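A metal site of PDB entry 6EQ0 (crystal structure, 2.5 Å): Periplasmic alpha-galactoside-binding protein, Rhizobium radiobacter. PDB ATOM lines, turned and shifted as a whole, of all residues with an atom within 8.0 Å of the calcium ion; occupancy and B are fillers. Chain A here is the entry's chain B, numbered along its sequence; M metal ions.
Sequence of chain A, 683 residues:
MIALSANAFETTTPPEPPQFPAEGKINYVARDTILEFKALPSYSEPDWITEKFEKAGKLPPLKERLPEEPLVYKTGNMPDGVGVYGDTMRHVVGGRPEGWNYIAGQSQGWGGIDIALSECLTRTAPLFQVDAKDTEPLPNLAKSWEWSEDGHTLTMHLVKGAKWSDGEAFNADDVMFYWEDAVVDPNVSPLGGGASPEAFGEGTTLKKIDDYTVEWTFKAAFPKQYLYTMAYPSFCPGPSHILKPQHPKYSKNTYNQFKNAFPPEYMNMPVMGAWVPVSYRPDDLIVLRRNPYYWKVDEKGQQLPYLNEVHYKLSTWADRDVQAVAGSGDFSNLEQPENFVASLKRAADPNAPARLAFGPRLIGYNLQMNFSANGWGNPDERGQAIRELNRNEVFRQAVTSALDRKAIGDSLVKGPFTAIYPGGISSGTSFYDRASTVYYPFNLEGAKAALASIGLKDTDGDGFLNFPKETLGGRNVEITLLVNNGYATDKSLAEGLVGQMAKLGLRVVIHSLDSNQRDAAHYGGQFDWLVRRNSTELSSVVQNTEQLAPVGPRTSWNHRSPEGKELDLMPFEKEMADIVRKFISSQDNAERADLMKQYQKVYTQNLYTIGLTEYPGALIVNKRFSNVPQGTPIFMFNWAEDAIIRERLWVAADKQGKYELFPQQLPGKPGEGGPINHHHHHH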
ATOM      1  N   LYS A 457     -22.767  -3.698  -7.011  1.00  0.00           N
ATOM      2  CA  LYS A 457     -22.450  -3.893  -5.601  1.00  0.00           C
ATOM      3  C   LYS A 457     -22.648  -5.350  -5.288  1.00  0.00           C
ATOM      4  O   LYS A 457     -23.588  -5.978  -5.807  1.00  0.00           O
ATOM      5  CB  LYS A 457     -23.396  -3.014  -4.716  1.00  0.00           C
ATOM      6  CG  LYS A 457     -23.569  -3.433  -3.226  1.00  0.00           C
ATOM      7  CD  LYS A 457     -23.963  -2.289  -2.288  1.00  0.00           C
ATOM      8  CE  LYS A 457     -25.351  -1.752  -2.522  1.00  0.00           C
ATOM      9  NZ  LYS A 457     -25.822  -0.875  -1.413  1.00  0.00           N
ATOM     10  N   ASP A 458     -21.775  -5.879  -4.440  1.00  0.00           N
ATOM     11  CA  ASP A 458     -21.902  -7.215  -3.901  1.00  0.00           C
ATOM     12  C   ASP A 458     -23.108  -7.133  -2.945  1.00  0.00           C
ATOM     13  O   ASP A 458     -23.098  -6.347  -1.992  1.00  0.00           O
ATOM     14  CB  ASP A 458     -20.609  -7.597  -3.164  1.00  0.00           C
ATOM     15  CG  ASP A 458     -20.654  -8.850  -2.324  1.00  0.00           C
ATOM     16  OD1 ASP A 458     -21.412  -9.781  -2.692  1.00  0.00           O
ATOM     17  OD2 ASP A 458     -19.906  -8.924  -1.330  1.00  0.00           O
ATOM     18  N   THR A 459     -24.188  -7.885  -3.268  1.00  0.00           N
ATOM     19  CA  THR A 459     -25.423  -7.930  -2.476  1.00  0.00           C
ATOM     20  C   THR A 459     -25.597  -9.269  -1.725  1.00  0.00           C
ATOM     21  O   THR A 459     -26.380  -9.332  -0.788  1.00  0.00           O
ATOM     22  CB  THR A 459     -26.678  -7.554  -3.320  1.00  0.00           C
ATOM     23  OG1 THR A 459     -27.084  -8.670  -4.113  1.00  0.00           O
ATOM     24  CG2 THR A 459     -26.484  -6.311  -4.166  1.00  0.00           C
ATOM     25  N   ASP A 460     -24.892 -10.323  -2.154  1.00  0.00           N
ATOM     26  CA  ASP A 460     -24.972 -11.677  -1.556  1.00  0.00           C
ATOM     27  C   ASP A 460     -23.707 -12.071  -0.725  1.00  0.00           C
ATOM     28  O   ASP A 460     -23.602 -13.203  -0.220  1.00  0.00           O
ATOM     29  CB  ASP A 460     -25.333 -12.747  -2.621  1.00  0.00           C
ATOM     30  CG  ASP A 460     -24.678 -12.626  -3.991  1.00  0.00           C
ATOM     31  OD1 ASP A 460     -23.654 -11.928  -4.103  1.00  0.00           O
ATOM     32  OD2 ASP A 460     -25.181 -13.255  -4.956  1.00  0.00           O
ATOM     33  N   GLY A 461     -22.779 -11.110  -0.583  1.00  0.00           N
ATOM     34  CA  GLY A 461     -21.581 -11.179   0.260  1.00  0.00           C
ATOM     35  C   GLY A 461     -20.470 -12.101  -0.135  1.00  0.00           C
ATOM     36  O   GLY A 461     -19.625 -12.405   0.717  1.00  0.00           O
ATOM     37  N   ASP A 462     -20.417 -12.526  -1.410  1.00  0.00           N
ATOM     38  CA  ASP A 462     -19.420 -13.478  -1.907  1.00  0.00           C
ATOM     39  C   ASP A 462     -18.163 -12.824  -2.506  1.00  0.00           C
ATOM     40  O   ASP A 462     -17.228 -13.537  -2.873  1.00  0.00           O
ATOM     41  CB  ASP A 462     -20.056 -14.473  -2.892  1.00  0.00           C
ATOM     42  CG  ASP A 462     -20.622 -13.895  -4.179  1.00  0.00           C
ATOM     43  OD1 ASP A 462     -20.970 -12.687  -4.175  1.00  0.00           O
ATOM     44  OD2 ASP A 462     -20.761 -14.645  -5.158  1.00  0.00           O
ATOM     45  N   GLY A 463     -18.134 -11.502  -2.554  1.00  0.00           N
ATOM     46  CA  GLY A 463     -17.008 -10.713  -3.072  1.00  0.00           C
ATOM     47  C   GLY A 463     -17.194 -10.232  -4.498  1.00  0.00           C
ATOM     48  O   GLY A 463     -16.535  -9.279  -4.913  1.00  0.00           O
ATOM     49  N   PHE A 464     -18.086 -10.910  -5.252  1.00  0.00           N
ATOM     50  CA  PHE A 464     -18.351 -10.615  -6.662  1.00  0.00           C
ATOM     51  C   PHE A 464     -19.568  -9.759  -6.838  1.00  0.00           C
ATOM     52  O   PHE A 464     -20.627 -10.081  -6.299  1.00  0.00           O
ATOM     53  CB  PHE A 464     -18.411 -11.890  -7.495  1.00  0.00           C
ATOM     54  CG  PHE A 464     -17.048 -12.521  -7.559  1.00  0.00           C
ATOM     55  CD1 PHE A 464     -16.050 -11.976  -8.365  1.00  0.00           C
ATOM     56  CD2 PHE A 464     -16.736 -13.607  -6.760  1.00  0.00           C
ATOM     57  CE1 PHE A 464     -14.768 -12.516  -8.380  1.00  0.00           C
ATOM     58  CE2 PHE A 464     -15.457 -14.164  -6.791  1.00  0.00           C
ATOM     59  CZ  PHE A 464     -14.480 -13.606  -7.601  1.00  0.00           C
ATOM     60  N   LEU A 465     -19.400  -8.632  -7.550  1.00  0.00           N
ATOM     61  CA  LEU A 465     -20.424  -7.621  -7.819  1.00  0.00           C
ATOM     62  C   LEU A 465     -21.688  -8.164  -8.473  1.00  0.00           C
ATOM     63  O   LEU A 465     -21.630  -8.981  -9.387  1.00  0.00           O
ATOM     64  CB  LEU A 465     -19.833  -6.463  -8.685  1.00  0.00           C
ATOM     65  CG  LEU A 465     -18.606  -5.684  -8.170  1.00  0.00           C
ATOM     66  CD1 LEU A 465     -18.207  -4.629  -9.166  1.00  0.00           C
ATOM     67  CD2 LEU A 465     -18.846  -5.043  -6.801  1.00  0.00           C
ATOM     68  N   ASN A 466     -22.831  -7.678  -8.034  1.00  0.00           N
ATOM     69  CA  ASN A 466     -24.126  -8.091  -8.571  1.00  0.00           C
ATOM     70  C   ASN A 466     -24.697  -7.052  -9.558  1.00  0.00           C
ATOM     71  O   ASN A 466     -24.321  -5.871  -9.518  1.00  0.00           O
ATOM     72  CB  ASN A 466     -25.127  -8.391  -7.431  1.00  0.00           C
ATOM     73  CG  ASN A 466     -24.879  -9.700  -6.699  1.00  0.00           C
ATOM     74  OD1 ASN A 466     -25.717 -10.612  -6.729  1.00  0.00           O
ATOM     75  ND2 ASN A 466     -23.744  -9.818  -6.009  1.00  0.00           N
ATOM     76  N   PHE A 467     -25.589  -7.514 -10.458  1.00  0.00           N
ATOM     77  CA  PHE A 467     -26.313  -6.669 -11.403  1.00  0.00           C
ATOM     78  C   PHE A 467     -27.429  -5.996 -10.596  1.00  0.00           C
ATOM     79  O   PHE A 467     -27.871  -6.585  -9.605  1.00  0.00           O
ATOM     80  CB  PHE A 467     -26.979  -7.555 -12.485  1.00  0.00           C
ATOM     81  CG  PHE A 467     -26.134  -7.975 -13.666  1.00  0.00           C
ATOM     82  CD1 PHE A 467     -25.765  -7.049 -14.644  1.00  0.00           C
ATOM     83  CD2 PHE A 467     -25.782  -9.308 -13.844  1.00  0.00           C
ATOM     84  CE1 PHE A 467     -25.021  -7.454 -15.754  1.00  0.00           C
ATOM     85  CE2 PHE A 467     -25.017  -9.703 -14.946  1.00  0.00           C
ATOM     86  CZ  PHE A 467     -24.662  -8.777 -15.902  1.00  0.00           C
ATOM     87  N   GLY A 474     -30.892  -9.597 -10.576  1.00  0.00           N
ATOM     88  CA  GLY A 474     -29.886  -9.092  -9.651  1.00  0.00           C
ATOM     89  C   GLY A 474     -28.724 -10.030  -9.405  1.00  0.00           C
ATOM     90  O   GLY A 474     -28.015  -9.868  -8.416  1.00  0.00           O
ATOM     91  N   ARG A 475     -28.512 -10.989 -10.328  1.00  0.00           N
ATOM     92  CA  ARG A 475     -27.479 -12.001 -10.247  1.00  0.00           C
ATOM     93  C   ARG A 475     -26.088 -11.404 -10.405  1.00  0.00           C
ATOM     94  O   ARG A 475     -25.962 -10.302 -10.926  1.00  0.00           O
ATOM     95  CB  ARG A 475     -27.735 -13.122 -11.279  1.00  0.00           C
ATOM     96  CG  ARG A 475     -27.396 -12.747 -12.716  1.00  0.00           C
ATOM     97  CD  ARG A 475     -27.392 -13.943 -13.647  1.00  0.00           C
ATOM     98  NE  ARG A 475     -28.657 -14.060 -14.359  1.00  0.00           N
ATOM     99  CZ  ARG A 475     -28.854 -14.810 -15.448  1.00  0.00           C
ATOM    100  NH1 ARG A 475     -27.860 -15.507 -15.965  1.00  0.00           N
ATOM    101  NH2 ARG A 475     -30.049 -14.841 -16.021  1.00  0.00           N
ATOM    102  N   ASN A 476     -25.055 -12.139  -9.964  1.00  0.00           N
ATOM    103  CA  ASN A 476     -23.651 -11.755 -10.046  1.00  0.00           C
ATOM    104  C   ASN A 476     -23.277 -11.569 -11.500  1.00  0.00           C
ATOM    105  O   ASN A 476     -23.752 -12.317 -12.365  1.00  0.00           O
ATOM    106  CB  ASN A 476     -22.743 -12.853  -9.450  1.00  0.00           C
ATOM    107  CG  ASN A 476     -22.604 -12.948  -7.931  1.00  0.00           C
ATOM    108  OD1 ASN A 476     -22.713 -11.981  -7.185  1.00  0.00           O
ATOM    109  ND2 ASN A 476     -22.238 -14.117  -7.447  1.00  0.00           N
ATOM    110  N   VAL A 477     -22.437 -10.592 -11.769  1.00  0.00           N
ATOM    111  CA  VAL A 477     -21.938 -10.362 -13.108  1.00  0.00           C
ATOM    112  C   VAL A 477     -20.921 -11.494 -13.360  1.00  0.00           C
ATOM    113  O   VAL A 477     -20.204 -11.916 -12.456  1.00  0.00           O
ATOM    114  CB  VAL A 477     -21.335  -8.923 -13.295  1.00  0.00           C
ATOM    115  CG1 VAL A 477     -20.697  -8.746 -14.671  1.00  0.00           C
ATOM    116  CG2 VAL A 477     -22.364  -7.830 -13.036  1.00  0.00           C
ATOM    117  N   GLY A 505     -13.819  -7.152  -8.363  1.00  0.00           N
ATOM    118  CA  GLY A 505     -15.086  -7.791  -8.004  1.00  0.00           C
ATOM    119  C   GLY A 505     -15.892  -8.322  -9.170  1.00  0.00           C
ATOM    120  O   GLY A 505     -17.099  -8.549  -9.037  1.00  0.00           O
HETATM  121 CA    CA M   1     -21.944 -10.740  -4.543  1.00  0.00          CA
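The side-chain amide oxygen (OD1) of Asn 476 lies close to the side-chain carboxylate (OD1) of Asp 460. OD1 of Asp 458 sits close to N of Gly 461 (2.8 Å). The side-chain carboxylate (OD2) of Asp 458 lies within hydrogen-bond range of the backbone NH (N) of Gly 463 (3.4 Å). OD2 of Asp 462 sits at hydrogen-bond distance from ND2 of Asn 476 (2.8 Å). The side-chain amide oxygen (OD1) of Asn 476 lies close to the backbone carbonyl oxygen (O) of Phe 464 (3.0 Å). OD1 of Asn 476 sits close to OD1 of Asn 466, 3.3 Å away. ND2 of Asn 466 lies close to N of Thr 459, 3.4 Å away. OD1 of Asn 466 sits close to O of Gly 474 (2.9 Å).
The calcium ion is bound by OD1 of Asp 460 (2.1 Å), OD1 of Asp 458 (2.2 Å), OD1 of Asp 462 (2.2 Å), O of Phe 464 (2.3 Å) and ND2 of Asn 466 (2.5 Å). The calcium ion has five donor atoms within binding distance. Slightly farther from the calcium ion lies the side-chain amide oxygen (OD1) of Asn 476 (3.0 Å).
Thr 459 touches the calcium ion. Seven residues have an atom within 4 Å of the calcium ion: Asp 458, Thr 459, Asp 460, Asp 462, Phe 464, Asn 466 and Asn 476.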
